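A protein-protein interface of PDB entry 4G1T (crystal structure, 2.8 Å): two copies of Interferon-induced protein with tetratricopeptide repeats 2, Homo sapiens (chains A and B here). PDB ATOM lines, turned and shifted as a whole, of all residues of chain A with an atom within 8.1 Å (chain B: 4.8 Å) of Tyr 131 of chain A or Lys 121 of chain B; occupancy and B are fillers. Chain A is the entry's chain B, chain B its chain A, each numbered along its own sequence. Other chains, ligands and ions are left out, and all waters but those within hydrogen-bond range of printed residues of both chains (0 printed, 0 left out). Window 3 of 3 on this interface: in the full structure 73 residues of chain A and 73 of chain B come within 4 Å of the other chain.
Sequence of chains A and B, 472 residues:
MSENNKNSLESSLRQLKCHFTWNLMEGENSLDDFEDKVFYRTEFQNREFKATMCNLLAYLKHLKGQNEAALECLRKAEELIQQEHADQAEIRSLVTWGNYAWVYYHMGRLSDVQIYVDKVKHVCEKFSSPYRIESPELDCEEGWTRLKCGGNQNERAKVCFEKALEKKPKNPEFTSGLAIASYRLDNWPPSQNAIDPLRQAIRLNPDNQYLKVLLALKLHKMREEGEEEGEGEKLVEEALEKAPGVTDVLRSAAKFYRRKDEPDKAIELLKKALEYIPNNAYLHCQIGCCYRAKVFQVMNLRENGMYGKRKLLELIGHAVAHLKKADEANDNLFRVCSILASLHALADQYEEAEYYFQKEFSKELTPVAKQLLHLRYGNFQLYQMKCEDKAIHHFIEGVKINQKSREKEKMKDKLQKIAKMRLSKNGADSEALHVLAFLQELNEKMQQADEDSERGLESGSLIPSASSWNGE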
ATOM      1  N   SER A 128     -12.888  29.204  22.700  1.00  0.00           N
ATOM      2  CA  SER A 128     -14.297  29.534  22.881  1.00  0.00           C
ATOM      3  C   SER A 128     -15.179  28.286  22.807  1.00  0.00           C
ATOM      4  O   SER A 128     -14.920  27.355  22.034  1.00  0.00           O
ATOM      5  CB  SER A 128     -14.788  30.593  21.897  1.00  0.00           C
ATOM      6  OG  SER A 128     -16.056  31.086  22.317  1.00  0.00           O
ATOM      7  N   SER A 129     -16.213  28.284  23.640  1.00  0.00           N
ATOM      8  CA  SER A 129     -17.231  27.247  23.635  1.00  0.00           C
ATOM      9  C   SER A 129     -18.231  27.557  22.520  1.00  0.00           C
ATOM     10  O   SER A 129     -18.551  28.724  22.269  1.00  0.00           O
ATOM     11  CB  SER A 129     -17.910  27.192  25.014  1.00  0.00           C
ATOM     12  OG  SER A 129     -19.149  26.501  25.000  1.00  0.00           O
ATOM     13  N   PRO A 130     -18.690  26.514  21.819  1.00  0.00           N
ATOM     14  CA  PRO A 130     -19.609  26.651  20.687  1.00  0.00           C
ATOM     15  C   PRO A 130     -21.047  26.703  21.141  1.00  0.00           C
ATOM     16  O   PRO A 130     -21.930  26.985  20.332  1.00  0.00           O
ATOM     17  CB  PRO A 130     -19.366  25.374  19.893  1.00  0.00           C
ATOM     18  CG  PRO A 130     -18.888  24.382  20.916  1.00  0.00           C
ATOM     19  CD  PRO A 130     -18.157  25.147  21.957  1.00  0.00           C
ATOM     20  N   TYR A 131     -21.263  26.439  22.428  1.00  0.00           N
ATOM     21  CA  TYR A 131     -22.605  26.320  23.013  1.00  0.00           C
ATOM     22  C   TYR A 131     -23.060  27.542  23.839  1.00  0.00           C
ATOM     23  O   TYR A 131     -24.253  27.867  23.871  1.00  0.00           O
ATOM     24  CB  TYR A 131     -22.691  25.075  23.897  1.00  0.00           C
ATOM     25  CG  TYR A 131     -22.219  23.788  23.261  1.00  0.00           C
ATOM     26  CD1 TYR A 131     -22.883  23.244  22.170  1.00  0.00           C
ATOM     27  CD2 TYR A 131     -21.126  23.097  23.772  1.00  0.00           C
ATOM     28  CE1 TYR A 131     -22.470  22.047  21.594  1.00  0.00           C
ATOM     29  CE2 TYR A 131     -20.701  21.896  23.200  1.00  0.00           C
ATOM     30  CZ  TYR A 131     -21.383  21.379  22.110  1.00  0.00           C
ATOM     31  OH  TYR A 131     -20.988  20.197  21.522  1.00  0.00           O
ATOM     32  N   ARG A 132     -22.115  28.205  24.507  1.00  0.00           N
ATOM     33  CA  ARG A 132     -22.425  29.353  25.350  1.00  0.00           C
ATOM     34  C   ARG A 132     -21.677  30.626  24.923  1.00  0.00           C
ATOM     35  O   ARG A 132     -20.616  30.560  24.298  1.00  0.00           O
ATOM     36  CB  ARG A 132     -22.114  29.008  26.805  1.00  0.00           C
ATOM     37  CG  ARG A 132     -20.737  28.413  27.020  1.00  0.00           C
ATOM     38  CD  ARG A 132     -20.626  27.747  28.382  1.00  0.00           C
ATOM     39  NE  ARG A 132     -20.878  28.687  29.467  1.00  0.00           N
ATOM     40  CZ  ARG A 132     -21.553  28.388  30.576  1.00  0.00           C
ATOM     41  NH1 ARG A 132     -22.048  27.168  30.745  1.00  0.00           N
ATOM     42  NH2 ARG A 132     -21.738  29.311  31.518  1.00  0.00           N
ATOM     43  N   ILE A 133     -22.247  31.785  25.249  1.00  0.00           N
ATOM     44  CA  ILE A 133     -21.544  33.068  25.104  1.00  0.00           C
ATOM     45  C   ILE A 133     -21.734  34.002  26.325  1.00  0.00           C
ATOM     46  O   ILE A 133     -22.744  33.937  27.022  1.00  0.00           O
ATOM     47  CB  ILE A 133     -21.917  33.794  23.789  1.00  0.00           C
ATOM     48  CG1 ILE A 133     -23.375  34.240  23.791  1.00  0.00           C
ATOM     49  CG2 ILE A 133     -21.655  32.890  22.616  1.00  0.00           C
ATOM     50  CD1 ILE A 133     -23.800  34.925  22.521  1.00  0.00           C
ATOM     51  N   LEU A 138     -27.764  38.118  28.284  1.00  0.00           N
ATOM     52  CA  LEU A 138     -27.941  36.776  28.832  1.00  0.00           C
ATOM     53  C   LEU A 138     -27.742  36.743  30.345  1.00  0.00           C
ATOM     54  O   LEU A 138     -27.973  35.713  30.998  1.00  0.00           O
ATOM     55  CB  LEU A 138     -26.932  35.798  28.216  1.00  0.00           C
ATOM     56  CG  LEU A 138     -27.030  35.359  26.761  1.00  0.00           C
ATOM     57  CD1 LEU A 138     -26.107  34.178  26.562  1.00  0.00           C
ATOM     58  CD2 LEU A 138     -28.461  35.005  26.350  1.00  0.00           C
ATOM     59  N   SER B  12     -22.744  17.965  26.487  1.00  0.00           N
ATOM     60  CA  SER B  12     -22.885  19.132  25.631  1.00  0.00           C
ATOM     61  C   SER B  12     -24.059  20.014  26.049  1.00  0.00           C
ATOM     62  O   SER B  12     -23.923  21.234  26.109  1.00  0.00           O
ATOM     63  CB  SER B  12     -23.033  18.714  24.177  1.00  0.00           C
ATOM     64  OG  SER B  12     -24.250  18.024  24.007  1.00  0.00           O
ATOM     65  N   GLN B  15     -23.549  22.560  28.946  1.00  0.00           N
ATOM     66  CA  GLN B  15     -22.843  23.820  28.685  1.00  0.00           C
ATOM     67  C   GLN B  15     -23.699  24.932  28.136  1.00  0.00           C
ATOM     68  O   GLN B  15     -23.240  26.071  28.041  1.00  0.00           O
ATOM     69  CB  GLN B  15     -21.707  23.621  27.697  1.00  0.00           C
ATOM     70  CG  GLN B  15     -20.641  22.695  28.181  1.00  0.00           C
ATOM     71  CD  GLN B  15     -19.498  22.597  27.205  1.00  0.00           C
ATOM     72  OE1 GLN B  15     -19.563  23.129  26.092  1.00  0.00           O
ATOM     73  NE2 GLN B  15     -18.428  21.915  27.619  1.00  0.00           N
ATOM     74  N   LEU B  16     -24.916  24.611  27.726  1.00  0.00           N
ATOM     75  CA  LEU B  16     -25.822  25.629  27.214  1.00  0.00           C
ATOM     76  C   LEU B  16     -26.290  26.516  28.355  1.00  0.00           C
ATOM     77  O   LEU B  16     -26.430  26.052  29.481  1.00  0.00           O
ATOM     78  CB  LEU B  16     -27.032  24.980  26.538  1.00  0.00           C
ATOM     79  CG  LEU B  16     -26.841  24.225  25.224  1.00  0.00           C
ATOM     80  CD1 LEU B  16     -28.170  23.649  24.755  1.00  0.00           C
ATOM     81  CD2 LEU B  16     -26.237  25.117  24.146  1.00  0.00           C
ATOM     82  N   LYS B  17     -26.516  27.793  28.074  1.00  0.00           N
ATOM     83  CA  LYS B  17     -27.113  28.683  29.060  1.00  0.00           C
ATOM     84  C   LYS B  17     -28.625  28.702  28.895  1.00  0.00           C
ATOM     85  O   LYS B  17     -29.147  29.246  27.922  1.00  0.00           O
ATOM     86  CB  LYS B  17     -26.607  30.133  28.898  1.00  0.00           C
ATOM     87  CG  LYS B  17     -25.216  30.449  29.436  1.00  0.00           C
ATOM     88  CD  LYS B  17     -24.943  31.941  29.294  1.00  0.00           C
ATOM     89  CE  LYS B  17     -23.590  32.352  29.858  1.00  0.00           C
ATOM     90  NZ  LYS B  17     -23.487  33.838  29.979  1.00  0.00           N
ATOM     91  N   GLN B 114     -30.944  17.754  18.474  1.00  0.00           N
ATOM     92  CA  GLN B 114     -29.891  18.132  17.529  1.00  0.00           C
ATOM     93  C   GLN B 114     -30.218  19.396  16.715  1.00  0.00           C
ATOM     94  O   GLN B 114     -29.342  20.223  16.484  1.00  0.00           O
ATOM     95  CB  GLN B 114     -29.540  16.978  16.601  1.00  0.00           C
ATOM     96  CG  GLN B 114     -28.367  17.279  15.684  1.00  0.00           C
ATOM     97  CD  GLN B 114     -27.101  17.593  16.457  1.00  0.00           C
ATOM     98  OE1 GLN B 114     -26.772  16.923  17.443  1.00  0.00           O
ATOM     99  NE2 GLN B 114     -26.387  18.631  16.022  1.00  0.00           N
ATOM    100  N   VAL B 117     -29.521  22.440  19.268  1.00  0.00           N
ATOM    101  CA  VAL B 117     -28.102  22.598  19.512  1.00  0.00           C
ATOM    102  C   VAL B 117     -27.432  23.226  18.289  1.00  0.00           C
ATOM    103  O   VAL B 117     -26.377  23.851  18.391  1.00  0.00           O
ATOM    104  CB  VAL B 117     -27.446  21.262  19.844  1.00  0.00           C
ATOM    105  CG1 VAL B 117     -25.936  21.378  19.839  1.00  0.00           C
ATOM    106  CG2 VAL B 117     -27.913  20.795  21.190  1.00  0.00           C
ATOM    107  N   ASP B 118     -28.051  23.063  17.126  1.00  0.00           N
ATOM    108  CA  ASP B 118     -27.522  23.679  15.923  1.00  0.00           C
ATOM    109  C   ASP B 118     -27.906  25.147  15.899  1.00  0.00           C
ATOM    110  O   ASP B 118     -27.033  26.002  15.818  1.00  0.00           O
ATOM    111  CB  ASP B 118     -27.965  22.934  14.658  1.00  0.00           C
ATOM    112  CG  ASP B 118     -27.133  21.668  14.410  1.00  0.00           C
ATOM    113  OD1 ASP B 118     -26.225  21.404  15.234  1.00  0.00           O
ATOM    114  OD2 ASP B 118     -27.384  20.934  13.413  1.00  0.00           O
ATOM    115  N   LYS B 119     -29.194  25.453  16.011  1.00  0.00           N
ATOM    116  CA  LYS B 119     -29.607  26.860  16.057  1.00  0.00           C
ATOM    117  C   LYS B 119     -28.827  27.624  17.136  1.00  0.00           C
ATOM    118  O   LYS B 119     -28.560  28.818  16.985  1.00  0.00           O
ATOM    119  CB  LYS B 119     -31.114  26.997  16.276  1.00  0.00           C
ATOM    120  CG  LYS B 119     -31.934  25.817  15.760  1.00  0.00           C
ATOM    121  CD  LYS B 119     -33.358  26.247  15.534  1.00  0.00           C
ATOM    122  CE  LYS B 119     -33.373  27.534  14.732  1.00  0.00           C
ATOM    123  NZ  LYS B 119     -34.685  28.225  14.831  1.00  0.00           N
ATOM    124  N   VAL B 120     -28.451  26.937  18.216  1.00  0.00           N
ATOM    125  CA  VAL B 120     -27.596  27.541  19.240  1.00  0.00           C
ATOM    126  C   VAL B 120     -26.175  27.751  18.704  1.00  0.00           C
ATOM    127  O   VAL B 120     -25.738  28.893  18.547  1.00  0.00           O
ATOM    128  CB  VAL B 120     -27.576  26.732  20.575  1.00  0.00           C
ATOM    129  CG1 VAL B 120     -26.419  27.155  21.450  1.00  0.00           C
ATOM    130  CG2 VAL B 120     -28.852  26.953  21.324  1.00  0.00           C
ATOM    131  N   LYS B 121     -25.473  26.658  18.404  1.00  0.00           N
ATOM    132  CA  LYS B 121     -24.102  26.734  17.902  1.00  0.00           C
ATOM    133  C   LYS B 121     -23.932  27.814  16.853  1.00  0.00           C
ATOM    134  O   LYS B 121     -22.893  28.462  16.799  1.00  0.00           O
ATOM    135  CB  LYS B 121     -23.655  25.405  17.305  1.00  0.00           C
ATOM    136  CG  LYS B 121     -23.241  24.359  18.308  1.00  0.00           C
ATOM    137  CD  LYS B 121     -23.029  23.032  17.586  1.00  0.00           C
ATOM    138  CE  LYS B 121     -22.460  21.963  18.503  1.00  0.00           C
ATOM    139  NZ  LYS B 121     -22.538  20.599  17.914  1.00  0.00           N
ATOM    140  N   HIS B 122     -24.947  28.001  16.015  1.00  0.00           N
ATOM    141  CA  HIS B 122     -24.859  28.996  14.966  1.00  0.00           C
ATOM    142  C   HIS B 122     -24.743  30.372  15.581  1.00  0.00           C
ATOM    143  O   HIS B 122     -23.709  31.022  15.467  1.00  0.00           O
ATOM    144  CB  HIS B 122     -26.065  28.955  14.028  1.00  0.00           C
ATOM    145  CG  HIS B 122     -25.972  29.939  12.904  1.00  0.00           C
ATOM    146  ND1 HIS B 122     -25.152  29.746  11.811  1.00  0.00           N
ATOM    147  CD2 HIS B 122     -26.569  31.141  12.715  1.00  0.00           C
ATOM    148  CE1 HIS B 122     -25.262  30.775  10.990  1.00  0.00           C
ATOM    149  NE2 HIS B 122     -26.117  31.633  11.518  1.00  0.00           N
ATOM    150  N   VAL B 123     -25.811  30.803  16.239  1.00  0.00           N
ATOM    151  CA  VAL B 123     -25.849  32.107  16.886  1.00  0.00           C
ATOM    152  C   VAL B 123     -24.647  32.344  17.823  1.00  0.00           C
ATOM    153  O   VAL B 123     -24.246  33.482  18.057  1.00  0.00           O
ATOM    154  CB  VAL B 123     -27.180  32.295  17.628  1.00  0.00           C
ATOM    155  CG1 VAL B 123     -27.259  33.665  18.249  1.00  0.00           C
ATOM    156  CG2 VAL B 123     -28.337  32.086  16.661  1.00  0.00           C
ATOM    157  N   CYS B 124     -24.050  31.277  18.338  1.00  0.00           N
ATOM    158  CA  CYS B 124     -22.909  31.431  19.237  1.00  0.00           C
ATOM    159  C   CYS B 124     -21.586  31.724  18.528  1.00  0.00           C
ATOM    160  O   CYS B 124     -20.749  32.448  19.060  1.00  0.00           O
ATOM    161  CB  CYS B 124     -22.766  30.225  20.174  1.00  0.00           C
ATOM    162  SG  CYS B 124     -23.787  30.352  21.660  1.00  0.00           S
ATOM    163  N   GLU B 125     -21.387  31.161  17.343  1.00  0.00           N
ATOM    164  CA  GLU B 125     -20.175  31.460  16.590  1.00  0.00           C
ATOM    165  C   GLU B 125     -20.270  32.862  15.958  1.00  0.00           C
ATOM    166  O   GLU B 125     -19.255  33.528  15.737  1.00  0.00           O
ATOM    167  CB  GLU B 125     -19.878  30.359  15.555  1.00  0.00           C
ATOM    168  CG  GLU B 125     -19.703  30.837  14.115  1.00  0.00           C
ATOM    169  CD  GLU B 125     -20.901  30.501  13.227  1.00  0.00           C
ATOM    170  OE1 GLU B 125     -21.052  29.316  12.837  1.00  0.00           O
ATOM    171  OE2 GLU B 125     -21.690  31.424  12.910  1.00  0.00           O
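The backbone carbonyl oxygen (O) of Ile 133 of chain A sits at hydrogen-bond distance from the side-chain amino group (NZ) of Lys 17 of chain B (3.1 Å).
O of Gln 15 of chain B lies close to NH1 of Arg 132 of chain A (3.2 Å).
The side-chain sulfur (SG) of Cys 124 of chain B is in hydrogen-bond range of the backbone carbonyl oxygen (O) of Tyr 131 of chain A, at 3.4 Å.
The side-chain hydroxyl of Ser 129 of chain A sits close to the backbone NH of Arg 132 of chain A.
The side-chain hydroxyl (OG) of Ser 129 of chain A sits close to the backbone NH (N) of Tyr 131 of chain A.
Among the printed residues, merely in contact across the chains: Tyr 131 of chain A with Gln 15 of chain B (2.8 Å), Tyr 131 of chain A with Lys 121 of chain B (3.1 Å), Pro 130 of chain A with Lys 121 of chain B (3.3 Å), Tyr 131 of chain A with Val 120 of chain B (3.3 Å), Pro 130 of chain A with Cys 124 of chain B (3.3 Å), Tyr 131 of chain A with Leu 16 of chain B (3.4 Å), Ile 133 of chain A with Cys 124 of chain B (3.4 Å), Ser 129 of chain A with Gln 15 of chain B (3.6 Å), Tyr 131 of chain A with Ser 12 of chain B (3.7 Å), Leu 138 of chain A with Lys 17 of chain B (3.7 Å), Arg 132 of chain A with Cys 124 of chain B (3.9 Å), Arg 132 of chain A with Lys 17 of chain B (3.9 Å) and Tyr 131 of chain A with Val 117 of chain B (3.9 Å).
Of chain B, only Ser 12, Gln 15, Leu 16, Val 117, Val 120, Lys 121 and Cys 124 come within 4 Å of Tyr 131 of chain A.
Of chain A, only Pro 130 and Tyr 131 come within 4 Å of Lys 121 of chain B.
Printed residues of chain B within 4 Å of Pro 130 of chain A: Lys 121 (3.3 Å) and Cys 124 (3.3 Å).
Of the printed residues of chain A, Lys 17 of chain B touches Arg 132 (3.9 Å), Ile 133 (3.1 Å) and Leu 138 (3.7 Å).
Printed residues of chain B within 4 Å of Leu 138 of chain A: Lys 17 (3.7 Å).
Printed residues of chain A within 4 Å of Cys 124 of chain B: Pro 130, Tyr 131, Arg 132 and Ile 133.
Of the printed residues of chain B, Arg 132 of chain A touches Gln 15 (3.1 Å), Lys 17 (3.9 Å) and Cys 124 (3.9 Å).
The nearest printed residue of chain B that does not touch Tyr 131 of chain A is Lys 17 of chain B (4.8 Å).
Of the 7 printed residues of chain A, 6 touch a printed residue of chain B.
Printed residues of chain B that touch a printed residue of chain A: Ser 12, Gln 15, Leu 16, Lys 17, Val 117, Val 120, Lys 121 and Cys 124.
Hydrophobic or aromatic side chains of chain B that line the printed part of chain A: Leu 16, Val 117 and Val 120.
Among the printed residues, no Asp or Glu carboxylate lies within 4 Å of a Lys or Arg side-chain nitrogen of the other chain.
No position is printed for both chains.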
